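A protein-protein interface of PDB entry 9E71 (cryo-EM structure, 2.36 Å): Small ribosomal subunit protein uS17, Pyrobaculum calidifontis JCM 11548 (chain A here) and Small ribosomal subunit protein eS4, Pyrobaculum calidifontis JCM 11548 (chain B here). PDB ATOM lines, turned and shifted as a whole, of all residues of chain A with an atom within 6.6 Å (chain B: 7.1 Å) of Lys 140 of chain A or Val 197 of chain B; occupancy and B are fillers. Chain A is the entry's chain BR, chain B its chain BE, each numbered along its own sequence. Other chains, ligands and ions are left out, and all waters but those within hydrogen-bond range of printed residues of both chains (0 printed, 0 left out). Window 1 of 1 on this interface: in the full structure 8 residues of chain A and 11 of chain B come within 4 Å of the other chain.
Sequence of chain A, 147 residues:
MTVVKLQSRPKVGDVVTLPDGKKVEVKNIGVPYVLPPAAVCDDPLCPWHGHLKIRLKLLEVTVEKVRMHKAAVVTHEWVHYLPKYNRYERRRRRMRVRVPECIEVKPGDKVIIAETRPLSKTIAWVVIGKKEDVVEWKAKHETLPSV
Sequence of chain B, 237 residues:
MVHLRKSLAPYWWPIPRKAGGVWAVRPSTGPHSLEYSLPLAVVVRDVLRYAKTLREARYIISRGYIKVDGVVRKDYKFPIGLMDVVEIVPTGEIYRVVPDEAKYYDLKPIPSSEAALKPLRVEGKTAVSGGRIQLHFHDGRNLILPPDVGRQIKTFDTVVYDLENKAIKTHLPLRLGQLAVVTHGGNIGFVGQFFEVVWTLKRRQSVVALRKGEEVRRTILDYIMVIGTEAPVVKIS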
ATOM      1  N   TRP A 137      19.495  29.989   4.849  1.00  0.00           N
ATOM      2  CA  TRP A 137      20.109  28.993   5.711  1.00  0.00           C
ATOM      3  C   TRP A 137      21.051  28.123   4.896  1.00  0.00           C
ATOM      4  O   TRP A 137      20.737  27.746   3.765  1.00  0.00           O
ATOM      5  CB  TRP A 137      19.049  28.120   6.382  1.00  0.00           C
ATOM      6  CG  TRP A 137      19.568  27.326   7.523  1.00  0.00           C
ATOM      7  CD1 TRP A 137      19.744  27.755   8.804  1.00  0.00           C
ATOM      8  CD2 TRP A 137      19.978  25.957   7.496  1.00  0.00           C
ATOM      9  NE1 TRP A 137      20.242  26.737   9.578  1.00  0.00           N
ATOM     10  CE2 TRP A 137      20.395  25.622   8.797  1.00  0.00           C
ATOM     11  CE3 TRP A 137      20.034  24.982   6.497  1.00  0.00           C
ATOM     12  CZ2 TRP A 137      20.856  24.355   9.127  1.00  0.00           C
ATOM     13  CZ3 TRP A 137      20.495  23.727   6.826  1.00  0.00           C
ATOM     14  CH2 TRP A 137      20.900  23.423   8.129  1.00  0.00           C
ATOM     15  N   LYS A 138      22.204  27.805   5.476  1.00  0.00           N
ATOM     16  CA  LYS A 138      23.184  26.943   4.836  1.00  0.00           C
ATOM     17  C   LYS A 138      23.712  25.934   5.845  1.00  0.00           C
ATOM     18  O   LYS A 138      23.779  26.209   7.045  1.00  0.00           O
ATOM     19  CB  LYS A 138      24.343  27.751   4.246  1.00  0.00           C
ATOM     20  CG  LYS A 138      24.096  28.245   2.832  1.00  0.00           C
ATOM     21  CD  LYS A 138      24.451  27.186   1.799  1.00  0.00           C
ATOM     22  CE  LYS A 138      23.842  27.506   0.441  1.00  0.00           C
ATOM     23  NZ  LYS A 138      22.711  26.601   0.100  1.00  0.00           N
ATOM     24  N   ALA A 139      24.088  24.762   5.346  1.00  0.00           N
ATOM     25  CA  ALA A 139      24.618  23.724   6.211  1.00  0.00           C
ATOM     26  C   ALA A 139      26.018  24.097   6.692  1.00  0.00           C
ATOM     27  O   ALA A 139      26.625  25.073   6.242  1.00  0.00           O
ATOM     28  CB  ALA A 139      24.640  22.380   5.484  1.00  0.00           C
ATOM     29  N   LYS A 140      26.527  23.305   7.630  1.00  0.00           N
ATOM     30  CA  LYS A 140      27.858  23.511   8.183  1.00  0.00           C
ATOM     31  C   LYS A 140      28.857  22.707   7.366  1.00  0.00           C
ATOM     32  O   LYS A 140      28.648  21.517   7.111  1.00  0.00           O
ATOM     33  CB  LYS A 140      27.919  23.099   9.656  1.00  0.00           C
ATOM     34  CG  LYS A 140      27.394  24.136  10.659  1.00  0.00           C
ATOM     35  CD  LYS A 140      25.911  24.412  10.477  1.00  0.00           C
ATOM     36  CE  LYS A 140      25.104  23.136  10.618  1.00  0.00           C
ATOM     37  NZ  LYS A 140      23.790  23.237   9.939  1.00  0.00           N
ATOM     38  N   HIS A 141      29.940  23.359   6.959  1.00  0.00           N
ATOM     39  CA  HIS A 141      30.889  22.793   6.011  1.00  0.00           C
ATOM     40  C   HIS A 141      32.259  22.805   6.676  1.00  0.00           C
ATOM     41  O   HIS A 141      32.920  23.849   6.718  1.00  0.00           O
ATOM     42  CB  HIS A 141      30.888  23.608   4.720  1.00  0.00           C
ATOM     43  CG  HIS A 141      31.029  22.790   3.474  1.00  0.00           C
ATOM     44  ND1 HIS A 141      31.834  21.676   3.386  1.00  0.00           N
ATOM     45  CD2 HIS A 141      30.452  22.932   2.256  1.00  0.00           C
ATOM     46  CE1 HIS A 141      31.748  21.169   2.169  1.00  0.00           C
ATOM     47  NE2 HIS A 141      30.916  21.912   1.465  1.00  0.00           N
ATOM     48  N   GLU A 142      32.685  21.659   7.200  1.00  0.00           N
ATOM     49  CA  GLU A 142      33.962  21.546   7.893  1.00  0.00           C
ATOM     50  C   GLU A 142      34.851  20.519   7.210  1.00  0.00           C
ATOM     51  O   GLU A 142      34.397  19.430   6.847  1.00  0.00           O
ATOM     52  CB  GLU A 142      33.769  21.167   9.358  1.00  0.00           C
ATOM     53  CG  GLU A 142      33.007  22.191  10.164  1.00  0.00           C
ATOM     54  CD  GLU A 142      32.126  21.556  11.213  1.00  0.00           C
ATOM     55  OE1 GLU A 142      32.589  20.606  11.875  1.00  0.00           O
ATOM     56  OE2 GLU A 142      30.974  22.008  11.378  1.00  0.00           O
ATOM     57  N   THR A 143      36.124  20.871   7.048  1.00  0.00           N
ATOM     58  CA  THR A 143      37.098  20.019   6.383  1.00  0.00           C
ATOM     59  C   THR A 143      38.380  19.978   7.200  1.00  0.00           C
ATOM     60  O   THR A 143      38.682  20.901   7.958  1.00  0.00           O
ATOM     61  CB  THR A 143      37.397  20.515   4.961  1.00  0.00           C
ATOM     62  OG1 THR A 143      36.191  21.000   4.360  1.00  0.00           O
ATOM     63  CG2 THR A 143      37.975  19.403   4.108  1.00  0.00           C
ATOM     64  N   LEU B 176      36.313  14.850  13.974  1.00  0.00           N
ATOM     65  CA  LEU B 176      36.963  14.888  12.674  1.00  0.00           C
ATOM     66  C   LEU B 176      38.393  14.376  12.796  1.00  0.00           C
ATOM     67  O   LEU B 176      39.119  14.748  13.722  1.00  0.00           O
ATOM     68  CB  LEU B 176      36.952  16.309  12.120  1.00  0.00           C
ATOM     69  CG  LEU B 176      35.820  16.636  11.149  1.00  0.00           C
ATOM     70  CD1 LEU B 176      35.789  18.125  10.845  1.00  0.00           C
ATOM     71  CD2 LEU B 176      35.952  15.827   9.884  1.00  0.00           C
ATOM     72  N   PHE B 194      38.004  10.229   8.773  1.00  0.00           N
ATOM     73  CA  PHE B 194      36.890  11.166   8.754  1.00  0.00           C
ATOM     74  C   PHE B 194      37.475  12.568   8.680  1.00  0.00           C
ATOM     75  O   PHE B 194      37.979  13.091   9.678  1.00  0.00           O
ATOM     76  CB  PHE B 194      36.013  10.988   9.989  1.00  0.00           C
ATOM     77  CG  PHE B 194      34.746  11.792   9.954  1.00  0.00           C
ATOM     78  CD1 PHE B 194      34.134  12.085   8.750  1.00  0.00           C
ATOM     79  CD2 PHE B 194      34.160  12.241  11.119  1.00  0.00           C
ATOM     80  CE1 PHE B 194      32.975  12.815   8.708  1.00  0.00           C
ATOM     81  CE2 PHE B 194      32.996  12.972  11.079  1.00  0.00           C
ATOM     82  CZ  PHE B 194      32.402  13.258   9.875  1.00  0.00           C
ATOM     83  N   PHE B 195      37.424  13.173   7.496  1.00  0.00           N
ATOM     84  CA  PHE B 195      38.064  14.458   7.273  1.00  0.00           C
ATOM     85  C   PHE B 195      37.126  15.555   6.803  1.00  0.00           C
ATOM     86  O   PHE B 195      37.565  16.706   6.712  1.00  0.00           O
ATOM     87  CB  PHE B 195      39.204  14.318   6.251  1.00  0.00           C
ATOM     88  CG  PHE B 195      38.743  14.321   4.823  1.00  0.00           C
ATOM     89  CD1 PHE B 195      38.094  13.226   4.295  1.00  0.00           C
ATOM     90  CD2 PHE B 195      38.959  15.420   4.012  1.00  0.00           C
ATOM     91  CE1 PHE B 195      37.669  13.224   2.988  1.00  0.00           C
ATOM     92  CE2 PHE B 195      38.529  15.422   2.707  1.00  0.00           C
ATOM     93  CZ  PHE B 195      37.886  14.322   2.195  1.00  0.00           C
ATOM     94  N   GLU B 196      35.868  15.252   6.496  1.00  0.00           N
ATOM     95  CA  GLU B 196      34.969  16.266   5.964  1.00  0.00           C
ATOM     96  C   GLU B 196      33.533  15.933   6.331  1.00  0.00           C
ATOM     97  O   GLU B 196      33.103  14.786   6.182  1.00  0.00           O
ATOM     98  CB  GLU B 196      35.106  16.380   4.446  1.00  0.00           C
ATOM     99  CG  GLU B 196      35.061  17.803   3.980  1.00  0.00           C
ATOM    100  CD  GLU B 196      33.656  18.272   3.709  1.00  0.00           C
ATOM    101  OE1 GLU B 196      32.821  17.470   3.245  1.00  0.00           O
ATOM    102  OE2 GLU B 196      33.371  19.436   4.041  1.00  0.00           O
ATOM    103  N   VAL B 197      32.792  16.935   6.794  1.00  0.00           N
ATOM    104  CA  VAL B 197      31.387  16.767   7.147  1.00  0.00           C
ATOM    105  C   VAL B 197      30.593  17.973   6.667  1.00  0.00           C
ATOM    106  O   VAL B 197      31.047  19.117   6.770  1.00  0.00           O
ATOM    107  CB  VAL B 197      31.192  16.554   8.663  1.00  0.00           C
ATOM    108  CG1 VAL B 197      31.487  17.826   9.431  1.00  0.00           C
ATOM    109  CG2 VAL B 197      29.776  16.089   8.947  1.00  0.00           C
ATOM    110  N   VAL B 198      29.421  17.704   6.106  1.00  0.00           N
ATOM    111  CA  VAL B 198      28.386  18.702   5.873  1.00  0.00           C
ATOM    112  C   VAL B 198      27.249  18.371   6.824  1.00  0.00           C
ATOM    113  O   VAL B 198      26.630  17.304   6.714  1.00  0.00           O
ATOM    114  CB  VAL B 198      27.904  18.705   4.414  1.00  0.00           C
ATOM    115  CG1 VAL B 198      26.682  19.579   4.268  1.00  0.00           C
ATOM    116  CG2 VAL B 198      29.008  19.179   3.489  1.00  0.00           C
ATOM    117  N   TRP B 199      26.986  19.268   7.767  1.00  0.00           N
ATOM    118  CA  TRP B 199      26.003  19.013   8.813  1.00  0.00           C
ATOM    119  C   TRP B 199      24.627  19.394   8.296  1.00  0.00           C
ATOM    120  O   TRP B 199      24.269  20.571   8.249  1.00  0.00           O
ATOM    121  CB  TRP B 199      26.345  19.788  10.077  1.00  0.00           C
ATOM    122  CG  TRP B 199      27.555  19.289  10.787  1.00  0.00           C
ATOM    123  CD1 TRP B 199      28.742  19.937  10.931  1.00  0.00           C
ATOM    124  CD2 TRP B 199      27.701  18.032  11.454  1.00  0.00           C
ATOM    125  NE1 TRP B 199      29.621  19.164  11.649  1.00  0.00           N
ATOM    126  CE2 TRP B 199      29.003  17.989  11.982  1.00  0.00           C
ATOM    127  CE3 TRP B 199      26.854  16.939  11.658  1.00  0.00           C
ATOM    128  CZ2 TRP B 199      29.479  16.898  12.698  1.00  0.00           C
ATOM    129  CZ3 TRP B 199      27.327  15.859  12.368  1.00  0.00           C
ATOM    130  CH2 TRP B 199      28.629  15.844  12.879  1.00  0.00           C
ATOM    131  N   THR B 200      23.850  18.395   7.902  1.00  0.00           N
ATOM    132  CA  THR B 200      22.467  18.635   7.536  1.00  0.00           C
ATOM    133  C   THR B 200      21.641  18.937   8.784  1.00  0.00           C
ATOM    134  O   THR B 200      22.111  18.806   9.917  1.00  0.00           O
ATOM    135  CB  THR B 200      21.896  17.428   6.798  1.00  0.00           C
ATOM    136  OG1 THR B 200      22.227  16.237   7.520  1.00  0.00           O
ATOM    137  CG2 THR B 200      22.480  17.341   5.407  1.00  0.00           C
ATOM    138  N   LEU B 201      20.396  19.368   8.561  1.00  0.00           N
ATOM    139  CA  LEU B 201      19.509  19.688   9.676  1.00  0.00           C
ATOM    140  C   LEU B 201      19.217  18.454  10.518  1.00  0.00           C
ATOM    141  O   LEU B 201      19.187  18.526  11.751  1.00  0.00           O
ATOM    142  CB  LEU B 201      18.212  20.301   9.157  1.00  0.00           C
ATOM    143  CG  LEU B 201      17.113  20.547  10.188  1.00  0.00           C
ATOM    144  CD1 LEU B 201      17.606  21.452  11.301  1.00  0.00           C
ATOM    145  CD2 LEU B 201      15.892  21.147   9.520  1.00  0.00           C
ATOM    146  N   SER B 206      23.634  13.659   7.879  1.00  0.00           N
ATOM    147  CA  SER B 206      24.757  14.516   7.535  1.00  0.00           C
ATOM    148  C   SER B 206      25.703  13.795   6.586  1.00  0.00           C
ATOM    149  O   SER B 206      25.868  12.575   6.645  1.00  0.00           O
ATOM    150  CB  SER B 206      25.506  14.944   8.792  1.00  0.00           C
ATOM    151  OG  SER B 206      24.609  15.157   9.863  1.00  0.00           O
ATOM    152  N   VAL B 207      26.332  14.563   5.704  1.00  0.00           N
ATOM    153  CA  VAL B 207      27.196  14.000   4.674  1.00  0.00           C
ATOM    154  C   VAL B 207      28.607  13.889   5.230  1.00  0.00           C
ATOM    155  O   VAL B 207      29.188  14.884   5.668  1.00  0.00           O
ATOM    156  CB  VAL B 207      27.174  14.856   3.401  1.00  0.00           C
ATOM    157  CG1 VAL B 207      27.799  14.100   2.249  1.00  0.00           C
ATOM    158  CG2 VAL B 207      25.756  15.258   3.067  1.00  0.00           C
ATOM    159  N   VAL B 208      29.168  12.685   5.209  1.00  0.00           N
ATOM    160  CA  VAL B 208      30.493  12.431   5.757  1.00  0.00           C
ATOM    161  C   VAL B 208      31.396  11.935   4.642  1.00  0.00           C
ATOM    162  O   VAL B 208      30.946  11.233   3.729  1.00  0.00           O
ATOM    163  CB  VAL B 208      30.446  11.417   6.917  1.00  0.00           C
ATOM    164  CG1 VAL B 208      29.344  11.789   7.888  1.00  0.00           C
ATOM    165  CG2 VAL B 208      30.245  10.010   6.388  1.00  0.00           C
ATOM    166  N   ALA B 209      32.668  12.315   4.709  1.00  0.00           N
ATOM    167  CA  ALA B 209      33.659  11.925   3.715  1.00  0.00           C
ATOM    168  C   ALA B 209      34.844  11.285   4.420  1.00  0.00           C
ATOM    169  O   ALA B 209      35.420  11.879   5.336  1.00  0.00           O
ATOM    170  CB  ALA B 209      34.112  13.130   2.893  1.00  0.00           C
ATOM    171  N   LEU B 221      26.123  10.208   7.747  1.00  0.00           N
ATOM    172  CA  LEU B 221      26.671  10.028   9.087  1.00  0.00           C
ATOM    173  C   LEU B 221      26.154   8.759   9.747  1.00  0.00           C
ATOM    174  O   LEU B 221      26.856   8.150  10.560  1.00  0.00           O
ATOM    175  CB  LEU B 221      26.343  11.242   9.952  1.00  0.00           C
ATOM    176  CG  LEU B 221      26.659  11.079  11.433  1.00  0.00           C
ATOM    177  CD1 LEU B 221      28.117  10.731  11.608  1.00  0.00           C
ATOM    178  CD2 LEU B 221      26.319  12.342  12.197  1.00  0.00           C
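N of Phe 195 of chain B lies close to O of Ala 209 of chain B, 3.2 Å away. The backbone NH of Val 198 of chain B sits at hydrogen-bond distance from the backbone carbonyl oxygen of Val 207 of chain B (2.9 Å). The backbone carbonyl oxygen of Glu 196 of chain B is in hydrogen-bond range of the backbone NH of Ala 209 of chain B (2.9 Å).
O of Glu 142 of chain A lies close to OE2 of Glu 196 of chain B, 3.0 Å away. The side-chain carboxylate of Glu 196 of chain B lies within hydrogen-bond range of a ring nitrogen (ND1) of His 141 of chain A (2.8 Å). The backbone NH (N) of Trp 199 of chain B lies within hydrogen-bond range of the backbone carbonyl oxygen (O) of Lys 140 of chain A (2.9 Å). OE2 of Glu 142 of chain A lies close to NE1 of Trp 199 of chain B. The backbone NH (N) of Val 197 of chain B is in hydrogen-bond range of the backbone carbonyl oxygen (O) of Glu 142 of chain A (3.0 Å). The backbone carbonyl oxygen (O) of Lys 140 of chain A sits close to the backbone carbonyl oxygen (O) of Val 197 of chain B (3.4 Å). The side-chain carboxylate of Glu 196 of chain B lies within hydrogen-bond range of the side-chain hydroxyl of Thr 143 of chain A (3.2 Å).
Of chain B, only Val 197, Val 198 and Trp 199 come within 4 Å of Lys 140 of chain A. Of chain A, only Lys 140, His 141 and Glu 142 come within 4 Å of Val 197 of chain B. Printed residues of chain A within 4 Å of Leu 176 of chain B: Glu 142. Printed residues of chain A within 4 Å of Trp 199 of chain B: Ala 139, Lys 140 and Glu 142. Of the printed residues of chain B, Ala 139 of chain A touches Val 198 (3.7 Å) and Trp 199 (3.3 Å). Printed residues of chain A within 4 Å of Val 198 of chain B: Ala 139 (3.7 Å), Lys 140 (3.1 Å) and His 141 (3.6 Å). Leu 221 of chain B touches none of the printed residues of chain A. The nearest residue of chain A that does not touch Val 197 of chain B is Thr 143 of chain A (5.2 Å). The nearest printed residue of chain B that does not touch Thr 143 of chain A is Leu 176 of chain B (4.7 Å).
Among the printed residues, pairs that only touch across the chains: Lys 140 of chain A with Val 198 of chain B (3.1 Å), Ala 139 of chain A with Trp 199 of chain B (3.3 Å), Thr 143 of chain A with Phe 195 of chain B (3.4 Å), His 141 of chain A with Val 198 of chain B (3.6 Å), Ala 139 of chain A with Val 198 of chain B (3.7 Å), His 141 of chain A with Val 197 of chain B (3.8 Å) and Glu 142 of chain A with Leu 176 of chain B (3.9 Å).
Of the 14 printed residues of chain B, 6 touch a printed residue of chain A. Along chain B the printed residues that touch a printed residue of chain A span positions 176 to 199. Of the 7 printed residues of chain A, 5 touch a printed residue of chain B. Hydrophobic or aromatic side chains of chain A that line the printed part of chain B: Ala 139 and His 141. Among the printed residues, no Asp or Glu carboxylate lies within 4 Å of a Lys or Arg side-chain nitrogen of the other chain.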
